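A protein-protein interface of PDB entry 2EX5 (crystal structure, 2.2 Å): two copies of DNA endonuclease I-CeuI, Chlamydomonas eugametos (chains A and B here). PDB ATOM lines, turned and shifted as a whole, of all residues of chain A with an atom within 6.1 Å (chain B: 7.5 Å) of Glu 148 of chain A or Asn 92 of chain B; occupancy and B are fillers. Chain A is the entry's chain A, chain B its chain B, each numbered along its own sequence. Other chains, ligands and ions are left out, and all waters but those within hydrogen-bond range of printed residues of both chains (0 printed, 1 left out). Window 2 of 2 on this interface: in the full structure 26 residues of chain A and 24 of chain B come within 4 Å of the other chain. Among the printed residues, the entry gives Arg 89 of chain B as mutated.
ND2 of Asn 92 of chain B sits at hydrogen-bond distance from OE1 of Glu 148 of chain A.
N of Leu 119 of chain B is in hydrogen-bond range of O of Arg 89 of chain B (2.8 Å).
N of Asn 92 of chain B lies within hydrogen-bond range of ND1 of His 90 of chain B (3.1 Å).
The side-chain carboxylate (OE2) of Glu 148 of chain A is in salt-bridge range of the side-chain amino group (NZ) of Lys 187 of chain A, 3.8 Å away.
O of Leu 2 of chain B is in hydrogen-bond range of ND2 of Asn 92 of chain B (2.9 Å).
The backbone NH of Lys 149 of chain A lies within hydrogen-bond range of the side-chain hydroxyl of Ser 146 of chain A.
Asn 92 of chain B touches Ser 146 of chain A.
Ser 146 of chain A touches Gly 93 of chain B (CB to CA, 3.9 Å).
N of Glu 148 of chain A touches CD1 of Ile 1 of chain B, 3.7 Å away.
Lys 149 of chain A touches Arg 89 of chain B.
Lys 151 of chain A touches Ile 1 of chain B.
Lys 187 of chain A touches Pro 4 of chain B.
Glu 148 of chain A touches two residues of chain B.
Asn 92 of chain B touches just these residues of chain A: Ser 146 (3.2 Å) and Glu 148 (3.2 Å).
Of the printed residues of chain B, Ser 146 of chain A touches Asn 92 and Gly 93.
Printed residues of chain A within 4 Å of Arg 89 of chain B: Lys 149 (3.7 Å).
Of the printed residues of chain B, Lys 187 of chain A touches Pro 4 (3.6 Å).
The nearest residue of chain B that does not touch Glu 148 of chain A is His 90 of chain B (5.5 Å).
Of the 9 printed residues of chain A, 5 touch a printed residue of chain B.
Of the 16 printed residues of chain B, 5 touch a printed residue of chain A.
Among the printed residues, 7 pairs touch across the chains.
No position is printed for both chains.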
ATOM      1  N   SER A 146      11.431  23.206  27.124  1.00  0.00           N
ATOM      2  CA  SER A 146      11.305  24.648  26.752  1.00  0.00           C
ATOM      3  C   SER A 146      10.703  24.754  25.378  1.00  0.00           C
ATOM      4  O   SER A 146      10.838  23.841  24.576  1.00  0.00           O
ATOM      5  CB  SER A 146      12.683  25.386  26.789  1.00  0.00           C
ATOM      6  OG  SER A 146      13.461  24.989  25.656  1.00  0.00           O
ATOM      7  N   PRO A 147       9.956  25.845  25.107  1.00  0.00           N
ATOM      8  CA  PRO A 147       9.515  26.061  23.746  1.00  0.00           C
ATOM      9  C   PRO A 147      10.516  25.841  22.619  1.00  0.00           C
ATOM     10  O   PRO A 147      10.152  25.234  21.630  1.00  0.00           O
ATOM     11  CB  PRO A 147       8.980  27.529  23.785  1.00  0.00           C
ATOM     12  CG  PRO A 147       8.291  27.570  25.197  1.00  0.00           C
ATOM     13  CD  PRO A 147       9.355  26.825  26.045  1.00  0.00           C
ATOM     14  N   GLU A 148      11.719  26.419  22.687  1.00  0.00           N
ATOM     15  CA  GLU A 148      12.739  26.177  21.663  1.00  0.00           C
ATOM     16  C   GLU A 148      13.010  24.709  21.424  1.00  0.00           C
ATOM     17  O   GLU A 148      13.190  24.322  20.315  1.00  0.00           O
ATOM     18  CB  GLU A 148      14.063  26.816  22.069  1.00  0.00           C
ATOM     19  CG  GLU A 148      14.932  26.928  20.861  1.00  0.00           C
ATOM     20  CD  GLU A 148      16.339  27.229  21.163  1.00  0.00           C
ATOM     21  OE1 GLU A 148      16.632  27.529  22.364  1.00  0.00           O
ATOM     22  OE2 GLU A 148      17.159  27.180  20.196  1.00  0.00           O
ATOM     23  N   LYS A 149      13.101  23.913  22.477  1.00  0.00           N
ATOM     24  CA  LYS A 149      13.656  22.543  22.302  1.00  0.00           C
ATOM     25  C   LYS A 149      12.555  21.717  21.681  1.00  0.00           C
ATOM     26  O   LYS A 149      12.837  20.955  20.815  1.00  0.00           O
ATOM     27  CB  LYS A 149      14.179  21.901  23.643  1.00  0.00           C
ATOM     28  CG  LYS A 149      15.707  21.818  23.916  1.00  0.00           C
ATOM     29  CD  LYS A 149      16.467  23.054  23.681  1.00  0.00           C
ATOM     30  CE  LYS A 149      17.927  22.757  23.272  1.00  0.00           C
ATOM     31  NZ  LYS A 149      18.791  22.398  24.410  1.00  0.00           N
ATOM     32  N   VAL A 150      11.301  21.930  22.113  1.00  0.00           N
ATOM     33  CA  VAL A 150      10.069  21.336  21.529  1.00  0.00           C
ATOM     34  C   VAL A 150       9.998  21.608  20.063  1.00  0.00           C
ATOM     35  O   VAL A 150       9.767  20.704  19.267  1.00  0.00           O
ATOM     36  CB  VAL A 150       8.714  21.858  22.236  1.00  0.00           C
ATOM     37  CG1 VAL A 150       7.426  21.338  21.580  1.00  0.00           C
ATOM     38  CG2 VAL A 150       8.738  21.572  23.659  1.00  0.00           C
ATOM     39  N   LYS A 151      10.212  22.841  19.670  1.00  0.00           N
ATOM     40  CA  LYS A 151      10.214  23.147  18.224  1.00  0.00           C
ATOM     41  C   LYS A 151      11.386  22.458  17.476  1.00  0.00           C
ATOM     42  O   LYS A 151      11.237  22.088  16.327  1.00  0.00           O
ATOM     43  CB  LYS A 151      10.260  24.690  18.046  1.00  0.00           C
ATOM     44  CG  LYS A 151      10.713  25.171  16.714  1.00  0.00           C
ATOM     45  CD  LYS A 151      11.050  26.713  16.842  1.00  0.00           C
ATOM     46  CE  LYS A 151      12.509  27.021  17.515  1.00  0.00           C
ATOM     47  NZ  LYS A 151      12.914  28.530  17.355  1.00  0.00           N
ATOM     48  N   ARG A 152      12.551  22.288  18.109  1.00  0.00           N
ATOM     49  CA  ARG A 152      13.687  21.579  17.421  1.00  0.00           C
ATOM     50  C   ARG A 152      13.292  20.137  17.195  1.00  0.00           C
ATOM     51  O   ARG A 152      13.492  19.564  16.153  1.00  0.00           O
ATOM     52  CB  ARG A 152      14.958  21.627  18.253  1.00  0.00           C
ATOM     53  CG  ARG A 152      15.563  22.979  18.342  1.00  0.00           C
ATOM     54  CD  ARG A 152      16.895  22.956  19.097  1.00  0.00           C
ATOM     55  NE  ARG A 152      17.965  22.343  18.327  1.00  0.00           N
ATOM     56  CZ  ARG A 152      18.729  22.957  17.403  1.00  0.00           C
ATOM     57  NH1 ARG A 152      19.713  22.296  16.788  1.00  0.00           N
ATOM     58  NH2 ARG A 152      18.523  24.221  17.092  1.00  0.00           N
ATOM     59  N   VAL A 153      12.660  19.544  18.182  1.00  0.00           N
ATOM     60  CA  VAL A 153      12.089  18.186  17.987  1.00  0.00           C
ATOM     61  C   VAL A 153      11.120  18.122  16.793  1.00  0.00           C
ATOM     62  O   VAL A 153      11.166  17.132  15.992  1.00  0.00           O
ATOM     63  CB  VAL A 153      11.388  17.601  19.320  1.00  0.00           C
ATOM     64  CG1 VAL A 153      10.553  16.317  19.004  1.00  0.00           C
ATOM     65  CG2 VAL A 153      12.487  17.298  20.432  1.00  0.00           C
ATOM     66  N   LYS A 187      22.620  26.883  15.011  1.00  0.00           N
ATOM     67  CA  LYS A 187      23.013  27.510  16.278  1.00  0.00           C
ATOM     68  C   LYS A 187      24.417  28.113  16.171  1.00  0.00           C
ATOM     69  O   LYS A 187      24.838  28.916  17.049  1.00  0.00           O
ATOM     70  CB  LYS A 187      23.133  26.398  17.301  1.00  0.00           C
ATOM     71  CG  LYS A 187      22.278  26.467  18.468  1.00  0.00           C
ATOM     72  CD  LYS A 187      20.906  26.264  18.166  1.00  0.00           C
ATOM     73  CE  LYS A 187      20.150  27.305  18.878  1.00  0.00           C
ATOM     74  NZ  LYS A 187      20.882  27.731  20.065  1.00  0.00           N
ATOM     75  N   ILE B   1      11.897  33.700  22.442  1.00  0.00           N
ATOM     76  CA  ILE B   1      12.992  32.775  21.923  1.00  0.00           C
ATOM     77  C   ILE B   1      14.070  33.554  21.151  1.00  0.00           C
ATOM     78  O   ILE B   1      13.987  33.766  19.923  1.00  0.00           O
ATOM     79  CB  ILE B   1      12.511  31.645  21.004  1.00  0.00           C
ATOM     80  CG1 ILE B   1      11.580  30.661  21.694  1.00  0.00           C
ATOM     81  CG2 ILE B   1      13.725  30.867  20.457  1.00  0.00           C
ATOM     82  CD1 ILE B   1      11.094  29.539  20.733  1.00  0.00           C
ATOM     83  N   LEU B   2      15.103  33.951  21.863  1.00  0.00           N
ATOM     84  CA  LEU B   2      16.129  34.751  21.251  1.00  0.00           C
ATOM     85  C   LEU B   2      17.357  33.952  20.706  1.00  0.00           C
ATOM     86  O   LEU B   2      17.845  32.954  21.299  1.00  0.00           O
ATOM     87  CB  LEU B   2      16.462  35.918  22.184  1.00  0.00           C
ATOM     88  CG  LEU B   2      17.355  35.799  23.371  1.00  0.00           C
ATOM     89  CD1 LEU B   2      18.757  35.926  22.832  1.00  0.00           C
ATOM     90  CD2 LEU B   2      17.054  36.957  24.250  1.00  0.00           C
ATOM     91  N   LYS B   3      17.822  34.384  19.539  1.00  0.00           N
ATOM     92  CA  LYS B   3      18.832  33.689  18.809  1.00  0.00           C
ATOM     93  C   LYS B   3      20.232  33.875  19.414  1.00  0.00           C
ATOM     94  O   LYS B   3      20.421  34.713  20.300  1.00  0.00           O
ATOM     95  CB  LYS B   3      18.752  34.096  17.338  1.00  0.00           C
ATOM     96  CG  LYS B   3      18.021  33.062  16.499  1.00  0.00           C
ATOM     97  CD  LYS B   3      18.017  33.395  14.962  1.00  0.00           C
ATOM     98  CE  LYS B   3      19.286  34.265  14.391  1.00  0.00           C
ATOM     99  NZ  LYS B   3      18.899  35.031  13.096  1.00  0.00           N
ATOM    100  N   PRO B   4      21.225  33.064  18.959  1.00  0.00           N
ATOM    101  CA  PRO B   4      22.616  33.221  19.393  1.00  0.00           C
ATOM    102  C   PRO B   4      23.184  34.665  19.200  1.00  0.00           C
ATOM    103  O   PRO B   4      22.862  35.332  18.217  1.00  0.00           O
ATOM    104  CB  PRO B   4      23.364  32.236  18.502  1.00  0.00           C
ATOM    105  CG  PRO B   4      22.354  31.302  18.017  1.00  0.00           C
ATOM    106  CD  PRO B   4      21.073  31.948  17.992  1.00  0.00           C
ATOM    107  N   LEU B   8      19.662  39.931  26.040  1.00  0.00           N
ATOM    108  CA  LEU B   8      18.463  40.245  26.856  1.00  0.00           C
ATOM    109  C   LEU B   8      18.303  41.754  26.880  1.00  0.00           C
ATOM    110  O   LEU B   8      19.251  42.456  27.266  1.00  0.00           O
ATOM    111  CB  LEU B   8      18.594  39.740  28.311  1.00  0.00           C
ATOM    112  CG  LEU B   8      17.870  38.432  28.609  1.00  0.00           C
ATOM    113  CD1 LEU B   8      18.301  37.853  30.004  1.00  0.00           C
ATOM    114  CD2 LEU B   8      16.317  38.530  28.414  1.00  0.00           C
ATOM    115  N   PHE B  40       8.696  36.350  31.769  1.00  0.00           N
ATOM    116  CA  PHE B  40       9.337  35.443  30.808  1.00  0.00           C
ATOM    117  C   PHE B  40       8.292  34.713  30.025  1.00  0.00           C
ATOM    118  O   PHE B  40       8.607  33.985  29.098  1.00  0.00           O
ATOM    119  CB  PHE B  40      10.308  34.484  31.517  1.00  0.00           C
ATOM    120  CG  PHE B  40      11.529  35.189  32.026  1.00  0.00           C
ATOM    121  CD1 PHE B  40      12.375  35.841  31.138  1.00  0.00           C
ATOM    122  CD2 PHE B  40      11.789  35.263  33.375  1.00  0.00           C
ATOM    123  CE1 PHE B  40      13.500  36.555  31.587  1.00  0.00           C
ATOM    124  CE2 PHE B  40      12.890  35.990  33.857  1.00  0.00           C
ATOM    125  CZ  PHE B  40      13.766  36.608  32.943  1.00  0.00           C
ATOM    126  N   ARG B  89      21.186  28.533  32.906  1.00  0.00           N
ATOM    127  CA  ARG B  89      20.477  28.171  31.712  1.00  0.00           C
ATOM    128  C   ARG B  89      20.250  29.483  30.955  1.00  0.00           C
ATOM    129  O   ARG B  89      19.982  30.456  31.568  1.00  0.00           O
ATOM    130  CB  ARG B  89      19.127  27.529  32.065  1.00  0.00           C
ATOM    131  CG  ARG B  89      18.371  26.975  30.898  1.00  0.00           C
ATOM    132  CD  ARG B  89      18.767  25.514  30.756  1.00  0.00           C
ATOM    133  NE  ARG B  89      18.106  24.833  29.650  1.00  0.00           N
ATOM    134  CZ  ARG B  89      18.719  23.896  28.902  1.00  0.00           C
ATOM    135  NH1 ARG B  89      20.022  23.529  29.162  1.00  0.00           N
ATOM    136  NH2 ARG B  89      18.053  23.330  27.889  1.00  0.00           N
ATOM    137  N   HIS B  90      20.419  29.451  29.643  1.00  0.00           N
ATOM    138  CA  HIS B  90      19.922  30.443  28.699  1.00  0.00           C
ATOM    139  C   HIS B  90      18.383  30.712  28.829  1.00  0.00           C
ATOM    140  O   HIS B  90      17.607  29.766  28.935  1.00  0.00           O
ATOM    141  CB  HIS B  90      20.216  29.959  27.282  1.00  0.00           C
ATOM    142  CG  HIS B  90      20.045  31.020  26.228  1.00  0.00           C
ATOM    143  ND1 HIS B  90      18.809  31.373  25.720  1.00  0.00           N
ATOM    144  CD2 HIS B  90      20.940  31.884  25.674  1.00  0.00           C
ATOM    145  CE1 HIS B  90      18.967  32.366  24.851  1.00  0.00           C
ATOM    146  NE2 HIS B  90      20.251  32.670  24.787  1.00  0.00           N
ATOM    147  N   VAL B  91      17.992  31.999  28.726  1.00  0.00           N
ATOM    148  CA  VAL B  91      16.601  32.453  28.856  1.00  0.00           C
ATOM    149  C   VAL B  91      15.651  31.550  28.164  1.00  0.00           C
ATOM    150  O   VAL B  91      14.637  31.236  28.738  1.00  0.00           O
ATOM    151  CB  VAL B  91      16.208  33.878  28.158  1.00  0.00           C
ATOM    152  CG1 VAL B  91      15.103  34.630  29.000  1.00  0.00           C
ATOM    153  CG2 VAL B  91      17.332  34.753  27.855  1.00  0.00           C
ATOM    154  N   ASN B  92      15.886  31.235  26.877  1.00  0.00           N
ATOM    155  CA  ASN B  92      15.066  30.229  26.153  1.00  0.00           C
ATOM    156  C   ASN B  92      14.680  29.023  26.957  1.00  0.00           C
ATOM    157  O   ASN B  92      13.564  28.455  26.680  1.00  0.00           O
ATOM    158  CB  ASN B  92      15.762  29.786  24.851  1.00  0.00           C
ATOM    159  CG  ASN B  92      15.999  30.963  23.936  1.00  0.00           C
ATOM    160  OD1 ASN B  92      15.614  32.105  24.294  1.00  0.00           O
ATOM    161  ND2 ASN B  92      16.608  30.723  22.777  1.00  0.00           N
ATOM    162  N   GLY B  93      15.532  28.672  27.947  1.00  0.00           N
ATOM    163  CA  GLY B  93      15.279  27.473  28.819  1.00  0.00           C
ATOM    164  C   GLY B  93      14.742  27.746  30.221  1.00  0.00           C
ATOM    165  O   GLY B  93      14.755  26.854  31.060  1.00  0.00           O
ATOM    166  N   VAL B  94      14.280  28.984  30.510  1.00  0.00           N
ATOM    167  CA  VAL B  94      13.820  29.338  31.872  1.00  0.00           C
ATOM    168  C   VAL B  94      12.689  28.467  32.413  1.00  0.00           C
ATOM    169  O   VAL B  94      12.502  28.390  33.615  1.00  0.00           O
ATOM    170  CB  VAL B  94      13.109  30.736  32.042  1.00  0.00           C
ATOM    171  CG1 VAL B  94      13.842  31.634  32.902  1.00  0.00           C
ATOM    172  CG2 VAL B  94      12.476  31.277  30.824  1.00  0.00           C
ATOM    173  N   LYS B  95      11.884  27.893  31.549  1.00  0.00           N
ATOM    174  CA  LYS B  95      10.804  27.053  31.983  1.00  0.00           C
ATOM    175  C   LYS B  95      11.300  26.056  32.978  1.00  0.00           C
ATOM    176  O   LYS B  95      10.591  25.778  33.910  1.00  0.00           O
ATOM    177  CB  LYS B  95      10.287  26.300  30.772  1.00  0.00           C
ATOM    178  CG  LYS B  95       8.899  25.907  30.899  1.00  0.00           C
ATOM    179  CD  LYS B  95       8.712  24.572  30.242  1.00  0.00           C
ATOM    180  CE  LYS B  95       7.280  24.240  30.160  1.00  0.00           C
ATOM    181  NZ  LYS B  95       7.197  23.343  29.020  1.00  0.00           N
ATOM    182  N   VAL B  96      12.516  25.518  32.794  1.00  0.00           N
ATOM    183  CA  VAL B  96      13.021  24.402  33.617  1.00  0.00           C
ATOM    184  C   VAL B  96      13.590  24.937  34.939  1.00  0.00           C
ATOM    185  O   VAL B  96      13.557  24.252  35.997  1.00  0.00           O
ATOM    186  CB  VAL B  96      14.041  23.554  32.810  1.00  0.00           C
ATOM    187  CG1 VAL B  96      14.497  22.324  33.592  1.00  0.00           C
ATOM    188  CG2 VAL B  96      13.417  23.086  31.460  1.00  0.00           C
ATOM    189  N   ALA B 117      22.497  36.426  27.592  1.00  0.00           N
ATOM    190  CA  ALA B 117      21.098  36.098  27.941  1.00  0.00           C
ATOM    191  C   ALA B 117      21.080  34.895  28.890  1.00  0.00           C
ATOM    192  O   ALA B 117      20.075  34.222  28.999  1.00  0.00           O
ATOM    193  CB  ALA B 117      20.281  35.808  26.718  1.00  0.00           C
ATOM    194  N   LEU B 119      20.714  32.997  32.377  1.00  0.00           N
ATOM    195  CA  LEU B 119      20.156  33.088  33.734  1.00  0.00           C
ATOM    196  C   LEU B 119      20.716  32.030  34.671  1.00  0.00           C
ATOM    197  O   LEU B 119      21.155  30.965  34.247  1.00  0.00           O
ATOM    198  CB  LEU B 119      18.603  33.019  33.718  1.00  0.00           C
ATOM    199  CG  LEU B 119      17.811  33.795  32.644  1.00  0.00           C
ATOM    200  CD1 LEU B 119      16.319  33.467  32.701  1.00  0.00           C
ATOM    201  CD2 LEU B 119      17.964  35.315  32.832  1.00  0.00           C
